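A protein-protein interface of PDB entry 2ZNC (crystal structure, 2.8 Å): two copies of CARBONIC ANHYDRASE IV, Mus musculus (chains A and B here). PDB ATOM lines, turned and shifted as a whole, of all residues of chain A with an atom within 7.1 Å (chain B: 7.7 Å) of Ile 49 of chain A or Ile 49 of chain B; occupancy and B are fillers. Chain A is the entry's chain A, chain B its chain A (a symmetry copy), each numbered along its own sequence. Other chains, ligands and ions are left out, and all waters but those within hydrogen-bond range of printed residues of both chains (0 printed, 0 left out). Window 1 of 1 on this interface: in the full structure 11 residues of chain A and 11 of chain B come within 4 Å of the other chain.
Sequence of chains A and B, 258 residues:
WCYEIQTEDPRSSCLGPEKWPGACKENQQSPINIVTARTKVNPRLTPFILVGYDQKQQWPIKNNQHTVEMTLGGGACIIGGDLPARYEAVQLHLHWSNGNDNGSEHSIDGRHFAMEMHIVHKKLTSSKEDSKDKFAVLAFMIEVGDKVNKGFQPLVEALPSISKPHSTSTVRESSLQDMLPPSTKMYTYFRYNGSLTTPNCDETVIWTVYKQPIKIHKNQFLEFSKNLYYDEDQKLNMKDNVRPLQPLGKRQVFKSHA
Among the printed residues, pairs that only touch across the chains: Val 51 of chain A with Tyr 187 of chain B (3.0 Å), Tyr 187 of chain A with Val 51 of chain B (3.0 Å), Pro 47 of chain A with Ile 49 of chain B (3.2 Å), Ile 49 of chain A with Pro 47 of chain B (3.2 Å), Ile 49 of chain A with Ile 49 of chain B (3.7 Å), Tyr 187 of chain A with Arg 86 of chain B (3.8 Å), Ile 79 of chain A with Tyr 187 of chain B (3.96 Å) and Tyr 187 of chain A with Ile 79 of chain B (3.96 Å).
The side-chain hydroxyl (OG) of Ser 183 of chain B lies within hydrogen-bond range of the backbone NH (N) of Gly 52 of chain A (3.2 Å).
Ile 49 of chain B touches just these residues of chain A: Pro 47 and Ile 49.
Printed residues of chain B within 4 Å of Gly 52 of chain A: Ser 183 (3.2 Å).
Of the printed residues of chain B, Val 51 of chain A touches Tyr 187 (3.0 Å).
Gly 81 of chain B touches none of the printed residues of chain A.
Tyr 53 of chain B touches none of the printed residues of chain A.
The nearest residue of chain B that does not touch Ile 49 of chain A is Phe 48 of chain B (4.1 Å).
The nearest residue of chain A that does not touch Ile 49 of chain B is Phe 48 of chain A (4.1 Å).
The nearest printed residue of chain A that does not touch Ile 79 of chain B is Pro 47 of chain A (4.6 Å).
Of the 20 printed residues of chain B, 7 touch a printed residue of chain A.
Hydrophobic or aromatic side chains of chain B within 4 Å of the printed part of chain A: Pro 47, Ile 49, Val 51, Ile 79 and Tyr 187.
Hydrophobic or aromatic side chains of chain A within 4 Å of the printed part of chain B: Pro 47, Ile 49, Val 51, Ile 79 and Tyr 187.
Along chain A the printed residues that touch a printed residue of chain B span positions 47 to 187.
Among the printed residues, no Asp or Glu carboxylate lies within 4 Å of a Lys or Arg side-chain nitrogen of the other chain.
Pro 47 of chain A touches Ile 49 of chain B, and with the chains exchanged Ile 49 of chain A touches Pro 47 of chain B.
Ile 49 of chain B touches its own counterpart, Ile 49 of chain A.
Val 51 of chain A touches Tyr 187 of chain B, and with the chains exchanged Tyr 187 of chain A touches Val 51 of chain B.
Ile 79 of chain A touches Tyr 187 of chain B, and with the chains exchanged Tyr 187 of chain A touches Ile 79 of chain B.
14 positions are printed for both chains.
N of Ile 49 of chain A sits at hydrogen-bond distance from O of Ile 79 of chain A (3.2 Å).
The backbone carbonyl oxygen (O) of Val 51 of chain A lies within hydrogen-bond range of the backbone NH (N) of Cys 77 of chain A, 2.8 Å away.
The backbone NH (N) of Ile 49 of chain B sits at hydrogen-bond distance from the backbone carbonyl oxygen (O) of Ile 79 of chain B (3.2 Å).
The backbone carbonyl oxygen (O) of Val 51 of chain B is in hydrogen-bond range of the backbone NH (N) of Cys 77 of chain B, at 2.8 Å.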
ATOM      1  N   THR A  46      24.671  -3.896  -8.115  1.00  0.00           N
ATOM      2  CA  THR A  46      24.827  -5.328  -7.893  1.00  0.00           C
ATOM      3  C   THR A  46      23.750  -6.054  -8.703  1.00  0.00           C
ATOM      4  O   THR A  46      22.735  -5.452  -9.059  1.00  0.00           O
ATOM      5  CB  THR A  46      24.686  -5.678  -6.395  1.00  0.00           C
ATOM      6  OG1 THR A  46      23.568  -4.976  -5.833  1.00  0.00           O
ATOM      7  CG2 THR A  46      25.954  -5.315  -5.646  1.00  0.00           C
ATOM      8  N   PRO A  47      23.958  -7.349  -9.012  1.00  0.00           N
ATOM      9  CA  PRO A  47      22.987  -8.129  -9.786  1.00  0.00           C
ATOM     10  C   PRO A  47      21.549  -7.981  -9.279  1.00  0.00           C
ATOM     11  O   PRO A  47      21.317  -7.821  -8.085  1.00  0.00           O
ATOM     12  CB  PRO A  47      23.503  -9.556  -9.619  1.00  0.00           C
ATOM     13  CG  PRO A  47      24.981  -9.361  -9.569  1.00  0.00           C
ATOM     14  CD  PRO A  47      25.121  -8.180  -8.644  1.00  0.00           C
ATOM     15  N   PHE A  48      20.599  -7.954 -10.207  1.00  0.00           N
ATOM     16  CA  PHE A  48      19.185  -7.821  -9.875  1.00  0.00           C
ATOM     17  C   PHE A  48      18.650  -9.077  -9.217  1.00  0.00           C
ATOM     18  O   PHE A  48      19.218 -10.157  -9.372  1.00  0.00           O
ATOM     19  CB  PHE A  48      18.352  -7.563 -11.135  1.00  0.00           C
ATOM     20  CG  PHE A  48      18.273  -6.122 -11.536  1.00  0.00           C
ATOM     21  CD1 PHE A  48      17.718  -5.180 -10.684  1.00  0.00           C
ATOM     22  CD2 PHE A  48      18.720  -5.707 -12.787  1.00  0.00           C
ATOM     23  CE1 PHE A  48      17.610  -3.845 -11.079  1.00  0.00           C
ATOM     24  CE2 PHE A  48      18.613  -4.378 -13.182  1.00  0.00           C
ATOM     25  CZ  PHE A  48      18.059  -3.451 -12.329  1.00  0.00           C
ATOM     26  N   ILE A  49      17.555  -8.918  -8.482  1.00  0.00           N
ATOM     27  CA  ILE A  49      16.888 -10.029  -7.828  1.00  0.00           C
ATOM     28  C   ILE A  49      15.710 -10.356  -8.745  1.00  0.00           C
ATOM     29  O   ILE A  49      14.806  -9.534  -8.918  1.00  0.00           O
ATOM     30  CB  ILE A  49      16.377  -9.630  -6.442  1.00  0.00           C
ATOM     31  CG1 ILE A  49      17.542  -9.150  -5.578  1.00  0.00           C
ATOM     32  CG2 ILE A  49      15.658 -10.804  -5.790  1.00  0.00           C
ATOM     33  CD1 ILE A  49      17.128  -8.502  -4.283  1.00  0.00           C
ATOM     34  N   LEU A  50      15.775 -11.517  -9.393  1.00  0.00           N
ATOM     35  CA  LEU A  50      14.737 -11.954 -10.325  1.00  0.00           C
ATOM     36  C   LEU A  50      13.646 -12.738  -9.630  1.00  0.00           C
ATOM     37  O   LEU A  50      13.864 -13.878  -9.218  1.00  0.00           O
ATOM     38  CB  LEU A  50      15.341 -12.817 -11.436  1.00  0.00           C
ATOM     39  CG  LEU A  50      16.403 -12.165 -12.317  1.00  0.00           C
ATOM     40  CD1 LEU A  50      16.932 -13.183 -13.289  1.00  0.00           C
ATOM     41  CD2 LEU A  50      15.834 -10.966 -13.061  1.00  0.00           C
ATOM     42  N   VAL A  51      12.468 -12.137  -9.516  1.00  0.00           N
ATOM     43  CA  VAL A  51      11.338 -12.796  -8.873  1.00  0.00           C
ATOM     44  C   VAL A  51      10.329 -13.275  -9.912  1.00  0.00           C
ATOM     45  O   VAL A  51       9.776 -12.474 -10.656  1.00  0.00           O
ATOM     46  CB  VAL A  51      10.612 -11.847  -7.897  1.00  0.00           C
ATOM     47  CG1 VAL A  51       9.387 -12.535  -7.312  1.00  0.00           C
ATOM     48  CG2 VAL A  51      11.552 -11.404  -6.794  1.00  0.00           C
ATOM     49  N   GLY A  52      10.085 -14.578  -9.955  1.00  0.00           N
ATOM     50  CA  GLY A  52       9.119 -15.119 -10.897  1.00  0.00           C
ATOM     51  C   GLY A  52       9.603 -15.443 -12.303  1.00  0.00           C
ATOM     52  O   GLY A  52       8.808 -15.851 -13.147  1.00  0.00           O
ATOM     53  N   TYR A  53      10.894 -15.257 -12.569  1.00  0.00           N
ATOM     54  CA  TYR A  53      11.447 -15.561 -13.889  1.00  0.00           C
ATOM     55  C   TYR A  53      11.558 -17.070 -14.085  1.00  0.00           C
ATOM     56  O   TYR A  53      11.634 -17.552 -15.211  1.00  0.00           O
ATOM     57  CB  TYR A  53      12.824 -14.902 -14.081  1.00  0.00           C
ATOM     58  CG  TYR A  53      12.777 -13.442 -14.496  1.00  0.00           C
ATOM     59  CD1 TYR A  53      12.077 -12.493 -13.734  1.00  0.00           C
ATOM     60  CD2 TYR A  53      13.424 -13.006 -15.657  1.00  0.00           C
ATOM     61  CE1 TYR A  53      12.021 -11.147 -14.122  1.00  0.00           C
ATOM     62  CE2 TYR A  53      13.374 -11.663 -16.055  1.00  0.00           C
ATOM     63  CZ  TYR A  53      12.669 -10.744 -15.284  1.00  0.00           C
ATOM     64  OH  TYR A  53      12.603  -9.428 -15.684  1.00  0.00           O
ATOM     65  N   CYS A  77       8.936  -9.959 -11.517  1.00  0.00           N
ATOM     66  CA  CYS A  77       9.367  -8.599 -11.226  1.00  0.00           C
ATOM     67  C   CYS A  77      10.818  -8.573 -10.741  1.00  0.00           C
ATOM     68  O   CYS A  77      11.425  -9.620 -10.513  1.00  0.00           O
ATOM     69  CB  CYS A  77       8.407  -7.911 -10.229  1.00  0.00           C
ATOM     70  SG  CYS A  77       8.604  -8.216  -8.440  1.00  0.00           S
ATOM     71  N   ILE A  78      11.397  -7.382 -10.677  1.00  0.00           N
ATOM     72  CA  ILE A  78      12.774  -7.230 -10.224  1.00  0.00           C
ATOM     73  C   ILE A  78      12.805  -6.291  -9.025  1.00  0.00           C
ATOM     74  O   ILE A  78      11.995  -5.365  -8.919  1.00  0.00           O
ATOM     75  CB  ILE A  78      13.708  -6.671 -11.345  1.00  0.00           C
ATOM     76  CG1 ILE A  78      13.142  -5.367 -11.915  1.00  0.00           C
ATOM     77  CG2 ILE A  78      13.909  -7.710 -12.439  1.00  0.00           C
ATOM     78  CD1 ILE A  78      14.055  -4.665 -12.872  1.00  0.00           C
ATOM     79  N   ILE A  79      13.723  -6.551  -8.108  1.00  0.00           N
ATOM     80  CA  ILE A  79      13.876  -5.740  -6.906  1.00  0.00           C
ATOM     81  C   ILE A  79      15.369  -5.469  -6.815  1.00  0.00           C
ATOM     82  O   ILE A  79      16.169  -6.245  -7.352  1.00  0.00           O
ATOM     83  CB  ILE A  79      13.446  -6.534  -5.625  1.00  0.00           C
ATOM     84  CG1 ILE A  79      12.015  -7.068  -5.770  1.00  0.00           C
ATOM     85  CG2 ILE A  79      13.550  -5.652  -4.395  1.00  0.00           C
ATOM     86  CD1 ILE A  79      11.660  -8.116  -4.777  1.00  0.00           C
ATOM     87  N   GLY A  80      15.752  -4.365  -6.181  1.00  0.00           N
ATOM     88  CA  GLY A  80      17.169  -4.072  -6.033  1.00  0.00           C
ATOM     89  C   GLY A  80      17.853  -3.483  -7.253  1.00  0.00           C
ATOM     90  O   GLY A  80      17.235  -2.741  -8.014  1.00  0.00           O
ATOM     91  N   GLY A  81      19.133  -3.804  -7.428  1.00  0.00           N
ATOM     92  CA  GLY A  81      19.892  -3.272  -8.550  1.00  0.00           C
ATOM     93  C   GLY A  81      19.909  -1.749  -8.524  1.00  0.00           C
ATOM     94  O   GLY A  81      19.775  -1.096  -9.561  1.00  0.00           O
ATOM     95  N   TYR A 187      26.537 -10.303 -14.315  1.00  0.00           N
ATOM     96  CA  TYR A 187      27.266  -9.479 -13.366  1.00  0.00           C
ATOM     97  C   TYR A 187      27.553  -8.117 -13.997  1.00  0.00           C
ATOM     98  O   TYR A 187      27.348  -7.075 -13.374  1.00  0.00           O
ATOM     99  CB  TYR A 187      28.613 -10.117 -13.033  1.00  0.00           C
ATOM    100  CG  TYR A 187      28.618 -11.146 -11.942  1.00  0.00           C
ATOM    101  CD1 TYR A 187      28.363 -10.788 -10.615  1.00  0.00           C
ATOM    102  CD2 TYR A 187      28.962 -12.469 -12.216  1.00  0.00           C
ATOM    103  CE1 TYR A 187      28.461 -11.725  -9.586  1.00  0.00           C
ATOM    104  CE2 TYR A 187      29.064 -13.415 -11.202  1.00  0.00           C
ATOM    105  CZ  TYR A 187      28.816 -13.038  -9.891  1.00  0.00           C
ATOM    106  OH  TYR A 187      28.946 -13.966  -8.881  1.00  0.00           O
ATOM    107  N   THR B  46      15.892  -8.233   2.231  1.00  0.00           N
ATOM    108  CA  THR B  46      15.283  -8.463   0.927  1.00  0.00           C
ATOM    109  C   THR B  46      15.797  -9.803   0.393  1.00  0.00           C
ATOM    110  O   THR B  46      16.846 -10.280   0.831  1.00  0.00           O
ATOM    111  CB  THR B  46      15.637  -7.331  -0.061  1.00  0.00           C
ATOM    112  OG1 THR B  46      17.033  -7.014   0.039  1.00  0.00           O
ATOM    113  CG2 THR B  46      14.805  -6.097   0.228  1.00  0.00           C
ATOM    114  N   PRO B  47      15.064 -10.430  -0.548  1.00  0.00           N
ATOM    115  CA  PRO B  47      15.472 -11.718  -1.119  1.00  0.00           C
ATOM    116  C   PRO B  47      16.941 -11.751  -1.552  1.00  0.00           C
ATOM    117  O   PRO B  47      17.491 -10.745  -1.987  1.00  0.00           O
ATOM    118  CB  PRO B  47      14.527 -11.864  -2.310  1.00  0.00           C
ATOM    119  CG  PRO B  47      13.279 -11.216  -1.812  1.00  0.00           C
ATOM    120  CD  PRO B  47      13.802  -9.966  -1.154  1.00  0.00           C
ATOM    121  N   PHE B  48      17.586 -12.894  -1.350  1.00  0.00           N
ATOM    122  CA  PHE B  48      18.988 -13.076  -1.714  1.00  0.00           C
ATOM    123  C   PHE B  48      19.167 -13.121  -3.218  1.00  0.00           C
ATOM    124  O   PHE B  48      18.226 -13.411  -3.954  1.00  0.00           O
ATOM    125  CB  PHE B  48      19.533 -14.388  -1.139  1.00  0.00           C
ATOM    126  CG  PHE B  48      20.034 -14.282   0.269  1.00  0.00           C
ATOM    127  CD1 PHE B  48      21.078 -13.428   0.585  1.00  0.00           C
ATOM    128  CD2 PHE B  48      19.486 -15.066   1.279  1.00  0.00           C
ATOM    129  CE1 PHE B  48      21.568 -13.362   1.891  1.00  0.00           C
ATOM    130  CE2 PHE B  48      19.973 -15.003   2.580  1.00  0.00           C
ATOM    131  CZ  PHE B  48      21.012 -14.152   2.883  1.00  0.00           C
ATOM    132  N   ILE B  49      20.385 -12.828  -3.659  1.00  0.00           N
ATOM    133  CA  ILE B  49      20.737 -12.875  -5.066  1.00  0.00           C
ATOM    134  C   ILE B  49      21.462 -14.211  -5.231  1.00  0.00           C
ATOM    135  O   ILE B  49      22.534 -14.415  -4.655  1.00  0.00           O
ATOM    136  CB  ILE B  49      21.671 -11.724  -5.443  1.00  0.00           C
ATOM    137  CG1 ILE B  49      21.001 -10.388  -5.126  1.00  0.00           C
ATOM    138  CG2 ILE B  49      22.045 -11.812  -6.917  1.00  0.00           C
ATOM    139  CD1 ILE B  49      21.916  -9.195  -5.224  1.00  0.00           C
ATOM    140  N   LEU B  50      20.827 -15.140  -5.942  1.00  0.00           N
ATOM    141  CA  LEU B  50      21.382 -16.474  -6.163  1.00  0.00           C
ATOM    142  C   LEU B  50      22.244 -16.530  -7.405  1.00  0.00           C
ATOM    143  O   LEU B  50      21.730 -16.476  -8.523  1.00  0.00           O
ATOM    144  CB  LEU B  50      20.260 -17.508  -6.287  1.00  0.00           C
ATOM    145  CG  LEU B  50      19.332 -17.669  -5.085  1.00  0.00           C
ATOM    146  CD1 LEU B  50      18.255 -18.662  -5.422  1.00  0.00           C
ATOM    147  CD2 LEU B  50      20.105 -18.121  -3.855  1.00  0.00           C
ATOM    148  N   VAL B  51      23.550 -16.659  -7.211  1.00  0.00           N
ATOM    149  CA  VAL B  51      24.481 -16.732  -8.331  1.00  0.00           C
ATOM    150  C   VAL B  51      24.969 -18.164  -8.535  1.00  0.00           C
ATOM    151  O   VAL B  51      25.582 -18.743  -7.646  1.00  0.00           O
ATOM    152  CB  VAL B  51      25.711 -15.831  -8.103  1.00  0.00           C
ATOM    153  CG1 VAL B  51      26.703 -16.000  -9.245  1.00  0.00           C
ATOM    154  CG2 VAL B  51      25.288 -14.381  -7.975  1.00  0.00           C
ATOM    155  N   GLY B  52      24.703 -18.727  -9.706  1.00  0.00           N
ATOM    156  CA  GLY B  52      25.153 -20.079  -9.995  1.00  0.00           C
ATOM    157  C   GLY B  52      24.266 -21.232  -9.550  1.00  0.00           C
ATOM    158  O   GLY B  52      24.634 -22.392  -9.727  1.00  0.00           O
ATOM    159  N   TYR B  53      23.109 -20.931  -8.968  1.00  0.00           N
ATOM    160  CA  TYR B  53      22.186 -21.979  -8.526  1.00  0.00           C
ATOM    161  C   TYR B  53      21.491 -22.614  -9.726  1.00  0.00           C
ATOM    162  O   TYR B  53      20.980 -23.727  -9.637  1.00  0.00           O
ATOM    163  CB  TYR B  53      21.141 -21.423  -7.544  1.00  0.00           C
ATOM    164  CG  TYR B  53      21.617 -21.310  -6.106  1.00  0.00           C
ATOM    165  CD1 TYR B  53      22.774 -20.585  -5.779  1.00  0.00           C
ATOM    166  CD2 TYR B  53      20.918 -21.937  -5.070  1.00  0.00           C
ATOM    167  CE1 TYR B  53      23.222 -20.491  -4.455  1.00  0.00           C
ATOM    168  CE2 TYR B  53      21.358 -21.851  -3.742  1.00  0.00           C
ATOM    169  CZ  TYR B  53      22.510 -21.130  -3.445  1.00  0.00           C
ATOM    170  OH  TYR B  53      22.954 -21.060  -2.144  1.00  0.00           O
ATOM    171  N   CYS B  77      27.051 -18.953  -5.286  1.00  0.00           N
ATOM    172  CA  CYS B  77      27.226 -18.087  -4.129  1.00  0.00           C
ATOM    173  C   CYS B  77      26.045 -17.128  -3.973  1.00  0.00           C
ATOM    174  O   CYS B  77      25.170 -17.061  -4.838  1.00  0.00           O
ATOM    175  CB  CYS B  77      28.578 -17.339  -4.191  1.00  0.00           C
ATOM    176  SG  CYS B  77      28.714 -15.816  -5.188  1.00  0.00           S
ATOM    177  N   ILE B  78      25.971 -16.462  -2.828  1.00  0.00           N
ATOM    178  CA  ILE B  78      24.894 -15.516  -2.568  1.00  0.00           C
ATOM    179  C   ILE B  78      25.492 -14.148  -2.265  1.00  0.00           C
ATOM    180  O   ILE B  78      26.585 -14.041  -1.699  1.00  0.00           O
ATOM    181  CB  ILE B  78      23.991 -15.963  -1.374  1.00  0.00           C
ATOM    182  CG1 ILE B  78      24.840 -16.227  -0.127  1.00  0.00           C
ATOM    183  CG2 ILE B  78      23.172 -17.188  -1.753  1.00  0.00           C
ATOM    184  CD1 ILE B  78      24.047 -16.491   1.116  1.00  0.00           C
ATOM    185  N   ILE B  79      24.788 -13.104  -2.673  1.00  0.00           N
ATOM    186  CA  ILE B  79      25.230 -11.732  -2.455  1.00  0.00           C
ATOM    187  C   ILE B  79      24.005 -11.019  -1.905  1.00  0.00           C
ATOM    188  O   ILE B  79      22.875 -11.455  -2.156  1.00  0.00           O
ATOM    189  CB  ILE B  79      25.632 -11.042  -3.804  1.00  0.00           C
ATOM    190  CG1 ILE B  79      26.692 -11.868  -4.543  1.00  0.00           C
ATOM    191  CG2 ILE B  79      26.151  -9.640  -3.547  1.00  0.00           C
ATOM    192  CD1 ILE B  79      26.865 -11.487  -5.969  1.00  0.00           C
ATOM    193  N   GLY B  80      24.213  -9.958  -1.131  1.00  0.00           N
ATOM    194  CA  GLY B  80      23.079  -9.215  -0.605  1.00  0.00           C
ATOM    195  C   GLY B  80      22.388  -9.828   0.599  1.00  0.00           C
ATOM    196  O   GLY B  80      23.035 -10.466   1.429  1.00  0.00           O
ATOM    197  N   GLY B  81      21.077  -9.622   0.700  1.00  0.00           N
ATOM    198  CA  GLY B  81      20.321 -10.142   1.830  1.00  0.00           C
ATOM    199  C   GLY B  81      20.866  -9.603   3.146  1.00  0.00           C
ATOM    200  O   GLY B  81      20.979 -10.333   4.132  1.00  0.00           O
ATOM    201  N   ARG B  86      29.988 -11.071   0.406  1.00  0.00           N
ATOM    202  CA  ARG B  86      29.506 -12.113  -0.491  1.00  0.00           C
ATOM    203  C   ARG B  86      29.926 -13.460   0.079  1.00  0.00           C
ATOM    204  O   ARG B  86      31.046 -13.612   0.575  1.00  0.00           O
ATOM    205  CB  ARG B  86      30.085 -11.914  -1.894  1.00  0.00           C
ATOM    206  CG  ARG B  86      29.681 -10.598  -2.527  1.00  0.00           C
ATOM    207  CD  ARG B  86      30.452 -10.303  -3.803  1.00  0.00           C
ATOM    208  NE  ARG B  86      30.014  -9.045  -4.409  1.00  0.00           N
ATOM    209  CZ  ARG B  86      29.645  -8.914  -5.681  1.00  0.00           C
ATOM    210  NH1 ARG B  86      29.674  -9.961  -6.501  1.00  0.00           N
ATOM    211  NH2 ARG B  86      29.253  -7.731  -6.137  1.00  0.00           N
ATOM    212  N   TYR B  87      29.017 -14.426   0.033  1.00  0.00           N
ATOM    213  CA  TYR B  87      29.290 -15.752   0.561  1.00  0.00           C
ATOM    214  C   TYR B  87      29.297 -16.851  -0.509  1.00  0.00           C
ATOM    215  O   TYR B  87      28.367 -16.974  -1.305  1.00  0.00           O
ATOM    216  CB  TYR B  87      28.297 -16.072   1.677  1.00  0.00           C
ATOM    217  CG  TYR B  87      28.564 -15.305   2.954  1.00  0.00           C
ATOM    218  CD1 TYR B  87      28.390 -13.918   3.016  1.00  0.00           C
ATOM    219  CD2 TYR B  87      29.018 -15.965   4.099  1.00  0.00           C
ATOM    220  CE1 TYR B  87      28.666 -13.211   4.186  1.00  0.00           C
ATOM    221  CE2 TYR B  87      29.296 -15.265   5.268  1.00  0.00           C
ATOM    222  CZ  TYR B  87      29.120 -13.893   5.303  1.00  0.00           C
ATOM    223  OH  TYR B  87      29.427 -13.212   6.456  1.00  0.00           O
ATOM    224  N   HIS B 121      27.621 -21.494   3.663  1.00  0.00           N
ATOM    225  CA  HIS B 121      28.353 -20.556   2.820  1.00  0.00           C
ATOM    226  C   HIS B 121      29.519 -19.964   3.607  1.00  0.00           C
ATOM    227  O   HIS B 121      29.350 -19.494   4.728  1.00  0.00           O
ATOM    228  CB  HIS B 121      27.423 -19.432   2.336  1.00  0.00           C
ATOM    229  CG  HIS B 121      26.242 -19.912   1.549  1.00  0.00           C
ATOM    230  ND1 HIS B 121      26.064 -19.611   0.216  1.00  0.00           N
ATOM    231  CD2 HIS B 121      25.188 -20.687   1.900  1.00  0.00           C
ATOM    232  CE1 HIS B 121      24.957 -20.183  -0.221  1.00  0.00           C
ATOM    233  NE2 HIS B 121      24.406 -20.841   0.782  1.00  0.00           N
ATOM    234  N   SER B 183      11.000 -19.041  -6.419  1.00  0.00           N
ATOM    235  CA  SER B 183      11.430 -17.734  -5.940  1.00  0.00           C
ATOM    236  C   SER B 183      10.314 -16.877  -5.335  1.00  0.00           C
ATOM    237  O   SER B 183      10.559 -16.060  -4.439  1.00  0.00           O
ATOM    238  CB  SER B 183      12.139 -16.973  -7.057  1.00  0.00           C
ATOM    239  OG  SER B 183      11.353 -16.941  -8.238  1.00  0.00           O
ATOM    240  N   MET B 186      10.320 -17.413  -1.737  1.00  0.00           N
ATOM    241  CA  MET B 186      11.523 -17.082  -0.978  1.00  0.00           C
ATOM    242  C   MET B 186      11.577 -15.622  -0.530  1.00  0.00           C
ATOM    243  O   MET B 186      12.634 -14.998  -0.484  1.00  0.00           O
ATOM    244  CB  MET B 186      12.776 -17.486  -1.752  1.00  0.00           C
ATOM    245  CG  MET B 186      12.890 -18.987  -1.956  1.00  0.00           C
ATOM    246  SD  MET B 186      14.541 -19.471  -2.426  1.00  0.00           S
ATOM    247  CE  MET B 186      14.432 -19.369  -4.227  1.00  0.00           C
ATOM    248  N   TYR B 187      10.410 -15.089  -0.198  1.00  0.00           N
ATOM    249  CA  TYR B 187      10.278 -13.723   0.278  1.00  0.00           C
ATOM    250  C   TYR B 187      10.365 -13.710   1.804  1.00  0.00           C
ATOM    251  O   TYR B 187      11.077 -12.894   2.389  1.00  0.00           O
ATOM    252  CB  TYR B 187       8.911 -13.157  -0.101  1.00  0.00           C
ATOM    253  CG  TYR B 187       8.791 -12.552  -1.470  1.00  0.00           C
ATOM    254  CD1 TYR B 187       9.464 -11.373  -1.796  1.00  0.00           C
ATOM    255  CD2 TYR B 187       7.933 -13.109  -2.418  1.00  0.00           C
ATOM    256  CE1 TYR B 187       9.280 -10.757  -3.034  1.00  0.00           C
ATOM    257  CE2 TYR B 187       7.738 -12.508  -3.656  1.00  0.00           C
ATOM    258  CZ  TYR B 187       8.409 -11.333  -3.958  1.00  0.00           C
ATOM    259  OH  TYR B 187       8.193 -10.720  -5.172  1.00  0.00           O
ATOM    260  N   TYR B 210      13.895 -20.211   6.154  1.00  0.00           N
ATOM    261  CA  TYR B 210      12.738 -19.854   5.339  1.00  0.00           C
ATOM    262  C   TYR B 210      11.415 -20.409   5.848  1.00  0.00           C
ATOM    263  O   TYR B 210      11.343 -21.553   6.285  1.00  0.00           O
ATOM    264  CB  TYR B 210      12.948 -20.298   3.891  1.00  0.00           C
ATOM    265  CG  TYR B 210      13.983 -19.498   3.151  1.00  0.00           C
ATOM    266  CD1 TYR B 210      15.337 -19.811   3.251  1.00  0.00           C
ATOM    267  CD2 TYR B 210      13.614 -18.412   2.358  1.00  0.00           C
ATOM    268  CE1 TYR B 210      16.298 -19.062   2.581  1.00  0.00           C
ATOM    269  CE2 TYR B 210      14.568 -17.659   1.682  1.00  0.00           C
ATOM    270  CZ  TYR B 210      15.906 -17.990   1.799  1.00  0.00           C
ATOM    271  OH  TYR B 210      16.857 -17.257   1.133  1.00  0.00           O
